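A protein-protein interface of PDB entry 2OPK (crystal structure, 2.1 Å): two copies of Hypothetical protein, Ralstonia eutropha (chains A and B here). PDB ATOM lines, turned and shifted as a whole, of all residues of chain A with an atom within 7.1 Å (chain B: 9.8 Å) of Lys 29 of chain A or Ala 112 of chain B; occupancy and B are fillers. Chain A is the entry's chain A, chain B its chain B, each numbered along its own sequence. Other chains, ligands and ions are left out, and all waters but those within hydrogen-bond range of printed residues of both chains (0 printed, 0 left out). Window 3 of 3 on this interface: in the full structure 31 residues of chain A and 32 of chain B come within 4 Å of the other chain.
N of Ala 87 of chain B is in hydrogen-bond range of OD1 of Asp 54 of chain B (2.9 Å).
The backbone NH (N) of Asp 54 of chain B is in hydrogen-bond range of the backbone carbonyl oxygen (O) of Cys 109 of chain B (2.7 Å).
OD2 of Asp 54 of chain B is in hydrogen-bond range of NE2 of His 84 of chain B, 2.7 Å away.
His 84 of chain B touches Arg 28 of chain A (CE1 to NH2, 3.5 Å).
Arg 28 of chain A touches Asp 110 of chain B.
Arg 28 of chain A touches Ala 112 of chain B (CD to C, 3.6 Å).
Leu 31 of chain A touches Leu 31 of chain B (CD1 to CD1, 3.3 Å).
Leu 31 of chain A touches Cys 109 of chain B.
Leu 31 of chain A touches its own counterpart, Leu 31 of chain B.
Positions printed for both chains: 29, 30, 31, 53 and 110.
Of the 8 pairs that touch across the chains among the printed residues, 1 has its exchanged pair printed and touching as well.
Hydrophobic or aromatic side chains of chain B that line the printed part of chain A: Leu 31 and His 84.
Among the printed residues, 8 pairs touch across the chains.
Among the printed residues, Asp or Glu carboxylates within 4 Å of a Lys or Arg side-chain nitrogen of the other chain: Arg 28 of chain A with Asp 54 of chain B.
The guanidinium group (NE) of Arg 28 of chain A lies within salt-bridge range of the side-chain carboxylate (OD2) of Asp 54 of chain B (2.9 Å).
O of Ala 111 of chain B is in hydrogen-bond range of NE of Arg 28 of chain A (3.3 Å).
The backbone NH (N) of Lys 29 of chain A is in hydrogen-bond range of the backbone carbonyl oxygen (O) of Ala 112 of chain B (3.2 Å).
Lys 29 of chain A touches one residue of chain B.
Ala 87 of chain B touches none of the printed residues of chain A.
Printed residues of chain A within 4 Å of Cys 109 of chain B: Leu 31 (3.1 Å).
Printed residues of chain A within 4 Å of Asp 110 of chain B: Arg 28 (3.5 Å).
The nearest residue of chain B that does not touch Lys 29 of chain A is Asp 110 of chain B (4.8 Å).
The nearest residue of chain A that does not touch Ala 112 of chain B is Glu 27 of chain A (5.3 Å).
The nearest printed residue of chain A that does not touch Asp 110 of chain B is Lys 29 of chain A (4.8 Å).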
ATOM      1  N   GLU A  27       1.569  13.582  -3.527  1.00  0.00           N
ATOM      2  CA  GLU A  27       0.526  14.366  -4.125  1.00  0.00           C
ATOM      3  C   GLU A  27       0.141  15.503  -3.189  1.00  0.00           C
ATOM      4  O   GLU A  27      -0.188  15.271  -2.032  1.00  0.00           O
ATOM      5  CB  GLU A  27      -0.677  13.469  -4.439  1.00  0.00           C
ATOM      6  CG  GLU A  27      -0.379  12.470  -5.545  1.00  0.00           C
ATOM      7  CD  GLU A  27      -1.524  11.509  -5.779  1.00  0.00           C
ATOM      8  OE1 GLU A  27      -1.591  10.477  -5.059  1.00  0.00           O
ATOM      9  OE2 GLU A  27      -2.338  11.800  -6.695  1.00  0.00           O
ATOM     10  N   ARG A  28       0.234  16.732  -3.689  1.00  0.00           N
ATOM     11  CA  ARG A  28      -0.194  17.933  -2.954  1.00  0.00           C
ATOM     12  C   ARG A  28      -0.938  18.806  -3.948  1.00  0.00           C
ATOM     13  O   ARG A  28      -0.972  18.488  -5.133  1.00  0.00           O
ATOM     14  CB  ARG A  28       1.027  18.674  -2.374  1.00  0.00           C
ATOM     15  CG  ARG A  28       1.796  17.886  -1.305  1.00  0.00           C
ATOM     16  CD  ARG A  28       0.942  17.820  -0.053  1.00  0.00           C
ATOM     17  NE  ARG A  28       1.528  17.120   1.064  1.00  0.00           N
ATOM     18  CZ  ARG A  28       1.232  15.889   1.444  1.00  0.00           C
ATOM     19  NH1 ARG A  28       0.349  15.154   0.783  1.00  0.00           N
ATOM     20  NH2 ARG A  28       1.838  15.384   2.507  1.00  0.00           N
ATOM     21  N   LYS A  29      -1.568  19.876  -3.484  1.00  0.00           N
ATOM     22  CA  LYS A  29      -2.248  20.815  -4.385  1.00  0.00           C
ATOM     23  C   LYS A  29      -1.302  21.276  -5.474  1.00  0.00           C
ATOM     24  O   LYS A  29      -0.240  21.863  -5.199  1.00  0.00           O
ATOM     25  CB  LYS A  29      -2.804  22.044  -3.643  1.00  0.00           C
ATOM     26  N   GLY A  30      -1.681  20.952  -6.709  1.00  0.00           N
ATOM     27  CA  GLY A  30      -0.928  21.330  -7.892  1.00  0.00           C
ATOM     28  C   GLY A  30       0.403  20.638  -8.035  1.00  0.00           C
ATOM     29  O   GLY A  30       1.302  21.186  -8.684  1.00  0.00           O
ATOM     30  N   LEU A  31       0.543  19.457  -7.418  1.00  0.00           N
ATOM     31  CA  LEU A  31       1.823  18.739  -7.444  1.00  0.00           C
ATOM     32  C   LEU A  31       1.686  17.235  -7.386  1.00  0.00           C
ATOM     33  O   LEU A  31       0.996  16.721  -6.519  1.00  0.00           O
ATOM     34  CB  LEU A  31       2.712  19.139  -6.259  1.00  0.00           C
ATOM     35  CG  LEU A  31       4.059  18.389  -6.308  1.00  0.00           C
ATOM     36  CD1 LEU A  31       5.018  18.990  -7.325  1.00  0.00           C
ATOM     37  CD2 LEU A  31       4.639  18.369  -4.996  1.00  0.00           C
ATOM     38  N   LYS A  32       2.388  16.532  -8.277  1.00  0.00           N
ATOM     39  CA  LYS A  32       2.457  15.088  -8.220  1.00  0.00           C
ATOM     40  C   LYS A  32       3.867  14.648  -8.555  1.00  0.00           C
ATOM     41  O   LYS A  32       4.391  14.985  -9.619  1.00  0.00           O
ATOM     42  CB  LYS A  32       1.449  14.453  -9.187  1.00  0.00           C
ATOM     43  CG  LYS A  32       1.353  12.933  -9.106  1.00  0.00           C
ATOM     44  CD  LYS A  32       0.111  12.397  -9.797  1.00  0.00           C
ATOM     45  CE  LYS A  32       0.203  12.515 -11.300  1.00  0.00           C
ATOM     46  NZ  LYS A  32      -1.078  12.016 -11.947  1.00  0.00           N
ATOM     47  N   GLN A  53      -0.239  21.240 -17.157  1.00  0.00           N
ATOM     48  CA  GLN A  53       0.847  21.313 -16.173  1.00  0.00           C
ATOM     49  C   GLN A  53       2.219  21.208 -16.817  1.00  0.00           C
ATOM     50  O   GLN A  53       2.398  20.620 -17.895  1.00  0.00           O
ATOM     51  CB  GLN A  53       0.691  20.222 -15.103  1.00  0.00           C
ATOM     52  CG  GLN A  53      -0.361  20.507 -14.035  1.00  0.00           C
ATOM     53  CD  GLN A  53      -0.423  19.412 -12.958  1.00  0.00           C
ATOM     54  OE1 GLN A  53      -0.422  18.234 -13.288  1.00  0.00           O
ATOM     55  NE2 GLN A  53      -0.485  19.804 -11.668  1.00  0.00           N
ATOM     56  N   ASP A 110       2.309  23.242 -11.545  1.00  0.00           N
ATOM     57  CA  ASP A 110       1.686  24.348 -12.257  1.00  0.00           C
ATOM     58  C   ASP A 110       2.636  25.030 -13.205  1.00  0.00           C
ATOM     59  O   ASP A 110       3.850  25.015 -13.022  1.00  0.00           O
ATOM     60  CB  ASP A 110       1.058  25.328 -11.264  1.00  0.00           C
ATOM     61  CG  ASP A 110      -0.125  24.690 -10.493  1.00  0.00           C
ATOM     62  OD1 ASP A 110      -0.580  23.575 -10.872  1.00  0.00           O
ATOM     63  OD2 ASP A 110      -0.589  25.285  -9.504  1.00  0.00           O
ATOM     64  N   LYS B  29       5.705  28.812  -8.704  1.00  0.00           N
ATOM     65  CA  LYS B  29       5.038  29.247  -7.464  1.00  0.00           C
ATOM     66  C   LYS B  29       4.730  28.017  -6.589  1.00  0.00           C
ATOM     67  O   LYS B  29       4.089  27.067  -7.056  1.00  0.00           O
ATOM     68  CB  LYS B  29       3.726  30.006  -7.765  1.00  0.00           C
ATOM     69  N   GLY B  30       5.221  28.035  -5.346  1.00  0.00           N
ATOM     70  CA  GLY B  30       5.053  26.905  -4.411  1.00  0.00           C
ATOM     71  C   GLY B  30       5.859  25.647  -4.756  1.00  0.00           C
ATOM     72  O   GLY B  30       5.544  24.544  -4.260  1.00  0.00           O
ATOM     73  N   LEU B  31       6.879  25.776  -5.609  1.00  0.00           N
ATOM     74  CA  LEU B  31       7.594  24.596  -6.058  1.00  0.00           C
ATOM     75  C   LEU B  31       9.047  24.840  -6.401  1.00  0.00           C
ATOM     76  O   LEU B  31       9.365  25.758  -7.161  1.00  0.00           O
ATOM     77  CB  LEU B  31       6.920  23.974  -7.292  1.00  0.00           C
ATOM     78  CG  LEU B  31       7.655  22.686  -7.713  1.00  0.00           C
ATOM     79  CD1 LEU B  31       7.158  21.502  -6.915  1.00  0.00           C
ATOM     80  CD2 LEU B  31       7.517  22.488  -9.109  1.00  0.00           C
ATOM     81  N   PRO B  52       8.349  24.986   6.502  1.00  0.00           N
ATOM     82  CA  PRO B  52       6.898  25.057   6.323  1.00  0.00           C
ATOM     83  C   PRO B  52       6.413  24.370   5.037  1.00  0.00           C
ATOM     84  O   PRO B  52       5.224  24.258   4.840  1.00  0.00           O
ATOM     85  CB  PRO B  52       6.624  26.555   6.256  1.00  0.00           C
ATOM     86  CG  PRO B  52       7.918  27.157   5.775  1.00  0.00           C
ATOM     87  CD  PRO B  52       9.013  26.275   6.240  1.00  0.00           C
ATOM     88  N   GLN B  53       7.337  23.973   4.163  1.00  0.00           N
ATOM     89  CA  GLN B  53       7.029  23.176   2.968  1.00  0.00           C
ATOM     90  C   GLN B  53       7.358  21.688   3.188  1.00  0.00           C
ATOM     91  O   GLN B  53       8.170  21.322   4.050  1.00  0.00           O
ATOM     92  CB  GLN B  53       7.851  23.675   1.792  1.00  0.00           C
ATOM     93  CG  GLN B  53       7.451  25.018   1.191  1.00  0.00           C
ATOM     94  CD  GLN B  53       8.253  25.315  -0.066  1.00  0.00           C
ATOM     95  OE1 GLN B  53       9.479  25.489  -0.015  1.00  0.00           O
ATOM     96  NE2 GLN B  53       7.570  25.352  -1.206  1.00  0.00           N
ATOM     97  N   ASP B  54       6.695  20.822   2.422  1.00  0.00           N
ATOM     98  CA  ASP B  54       7.070  19.402   2.387  1.00  0.00           C
ATOM     99  C   ASP B  54       8.351  19.321   1.571  1.00  0.00           C
ATOM    100  O   ASP B  54       8.601  20.190   0.743  1.00  0.00           O
ATOM    101  CB  ASP B  54       6.013  18.569   1.676  1.00  0.00           C
ATOM    102  CG  ASP B  54       4.874  18.163   2.573  1.00  0.00           C
ATOM    103  OD1 ASP B  54       4.651  18.772   3.640  1.00  0.00           O
ATOM    104  OD2 ASP B  54       4.228  17.179   2.198  1.00  0.00           O
ATOM    105  N   GLU B  55       9.149  18.293   1.817  1.00  0.00           N
ATOM    106  CA  GLU B  55      10.328  17.972   1.011  1.00  0.00           C
ATOM    107  C   GLU B  55      10.281  16.496   0.643  1.00  0.00           C
ATOM    108  O   GLU B  55       9.875  15.656   1.464  1.00  0.00           O
ATOM    109  CB  GLU B  55      11.627  18.285   1.761  1.00  0.00           C
ATOM    110  CG  GLU B  55      12.886  18.042   0.902  1.00  0.00           C
ATOM    111  CD  GLU B  55      14.200  18.376   1.592  1.00  0.00           C
ATOM    112  OE1 GLU B  55      14.168  18.969   2.710  1.00  0.00           O
ATOM    113  OE2 GLU B  55      15.274  18.047   1.003  1.00  0.00           O
ATOM    114  N   HIS B  84      10.129  11.224   2.123  1.00  0.00           N
ATOM    115  CA  HIS B  84       9.212  12.344   2.165  1.00  0.00           C
ATOM    116  C   HIS B  84       9.240  12.898   3.596  1.00  0.00           C
ATOM    117  O   HIS B  84       8.969  12.175   4.547  1.00  0.00           O
ATOM    118  CB  HIS B  84       7.805  11.942   1.752  1.00  0.00           C
ATOM    119  CG  HIS B  84       6.778  12.994   2.042  1.00  0.00           C
ATOM    120  ND1 HIS B  84       5.606  12.730   2.715  1.00  0.00           N
ATOM    121  CD2 HIS B  84       6.771  14.324   1.780  1.00  0.00           C
ATOM    122  CE1 HIS B  84       4.916  13.852   2.840  1.00  0.00           C
ATOM    123  NE2 HIS B  84       5.610  14.838   2.297  1.00  0.00           N
ATOM    124  N   PRO B  86       7.398  15.612   5.723  1.00  0.00           N
ATOM    125  CA  PRO B  86       6.280  16.562   5.821  1.00  0.00           C
ATOM    126  C   PRO B  86       6.699  17.871   6.476  1.00  0.00           C
ATOM    127  O   PRO B  86       7.693  17.896   7.221  1.00  0.00           O
ATOM    128  CB  PRO B  86       5.279  15.837   6.716  1.00  0.00           C
ATOM    129  CG  PRO B  86       5.644  14.401   6.623  1.00  0.00           C
ATOM    130  CD  PRO B  86       7.111  14.385   6.496  1.00  0.00           C
ATOM    131  N   ALA B  87       5.956  18.945   6.199  1.00  0.00           N
ATOM    132  CA  ALA B  87       6.270  20.259   6.776  1.00  0.00           C
ATOM    133  C   ALA B  87       6.294  20.151   8.284  1.00  0.00           C
ATOM    134  O   ALA B  87       5.461  19.477   8.887  1.00  0.00           O
ATOM    135  CB  ALA B  87       5.285  21.282   6.347  1.00  0.00           C
ATOM    136  N   HIS B  88       7.301  20.775   8.865  1.00  0.00           N
ATOM    137  CA  HIS B  88       7.546  20.817  10.297  1.00  0.00           C
ATOM    138  C   HIS B  88       8.107  19.560  10.941  1.00  0.00           C
ATOM    139  O   HIS B  88       8.390  19.586  12.137  1.00  0.00           O
ATOM    140  CB  HIS B  88       6.374  21.441  11.051  1.00  0.00           C
ATOM    141  CG  HIS B  88       6.055  22.812  10.552  1.00  0.00           C
ATOM    142  ND1 HIS B  88       6.983  23.836  10.574  1.00  0.00           N
ATOM    143  CD2 HIS B  88       4.958  23.307   9.934  1.00  0.00           C
ATOM    144  CE1 HIS B  88       6.454  24.908  10.020  1.00  0.00           C
ATOM    145  NE2 HIS B  88       5.221  24.617   9.632  1.00  0.00           N
ATOM    146  N   HIS B 108      10.706  20.636  -3.114  1.00  0.00           N
ATOM    147  CA  HIS B 108      10.095  21.407  -2.069  1.00  0.00           C
ATOM    148  C   HIS B 108       8.752  21.869  -2.571  1.00  0.00           C
ATOM    149  O   HIS B 108       8.647  22.418  -3.649  1.00  0.00           O
ATOM    150  CB  HIS B 108      11.011  22.595  -1.735  1.00  0.00           C
ATOM    151  CG  HIS B 108      12.375  22.186  -1.248  1.00  0.00           C
ATOM    152  ND1 HIS B 108      12.646  21.901   0.080  1.00  0.00           N
ATOM    153  CD2 HIS B 108      13.538  21.985  -1.920  1.00  0.00           C
ATOM    154  CE1 HIS B 108      13.919  21.563   0.202  1.00  0.00           C
ATOM    155  NE2 HIS B 108      14.484  21.615  -0.993  1.00  0.00           N
ATOM    156  N   CYS B 109       7.706  21.625  -1.799  1.00  0.00           N
ATOM    157  CA  CYS B 109       6.375  22.016  -2.198  1.00  0.00           C
ATOM    158  C   CYS B 109       5.464  22.278  -1.000  1.00  0.00           C
ATOM    159  O   CYS B 109       5.830  21.972   0.149  1.00  0.00           O
ATOM    160  CB  CYS B 109       5.784  20.926  -3.074  1.00  0.00           C
ATOM    161  SG  CYS B 109       5.478  19.414  -2.216  1.00  0.00           S
ATOM    162  N   ASP B 110       4.265  22.805  -1.271  1.00  0.00           N
ATOM    163  CA  ASP B 110       3.291  23.160  -0.219  1.00  0.00           C
ATOM    164  C   ASP B 110       2.917  21.970   0.628  1.00  0.00           C
ATOM    165  O   ASP B 110       2.916  20.834   0.137  1.00  0.00           O
ATOM    166  CB  ASP B 110       2.009  23.764  -0.823  1.00  0.00           C
ATOM    167  CG  ASP B 110       2.247  25.123  -1.494  1.00  0.00           C
ATOM    168  OD1 ASP B 110       3.172  25.860  -1.093  1.00  0.00           O
ATOM    169  OD2 ASP B 110       1.508  25.452  -2.447  1.00  0.00           O
ATOM    170  N   ALA B 111       2.612  22.211   1.901  1.00  0.00           N
ATOM    171  CA  ALA B 111       2.133  21.134   2.771  1.00  0.00           C
ATOM    172  C   ALA B 111       0.701  20.790   2.342  1.00  0.00           C
ATOM    173  O   ALA B 111       0.190  19.703   2.652  1.00  0.00           O
ATOM    174  CB  ALA B 111       2.179  21.556   4.199  1.00  0.00           C
ATOM    175  N   ALA B 112       0.081  21.764   1.660  1.00  0.00           N
ATOM    176  CA  ALA B 112      -1.223  21.682   0.989  1.00  0.00           C
ATOM    177  C   ALA B 112      -1.211  20.731  -0.197  1.00  0.00           C
ATOM    178  O   ALA B 112      -2.112  19.902  -0.341  1.00  0.00           O
ATOM    179  CB  ALA B 112      -1.660  23.120   0.493  1.00  0.00           C
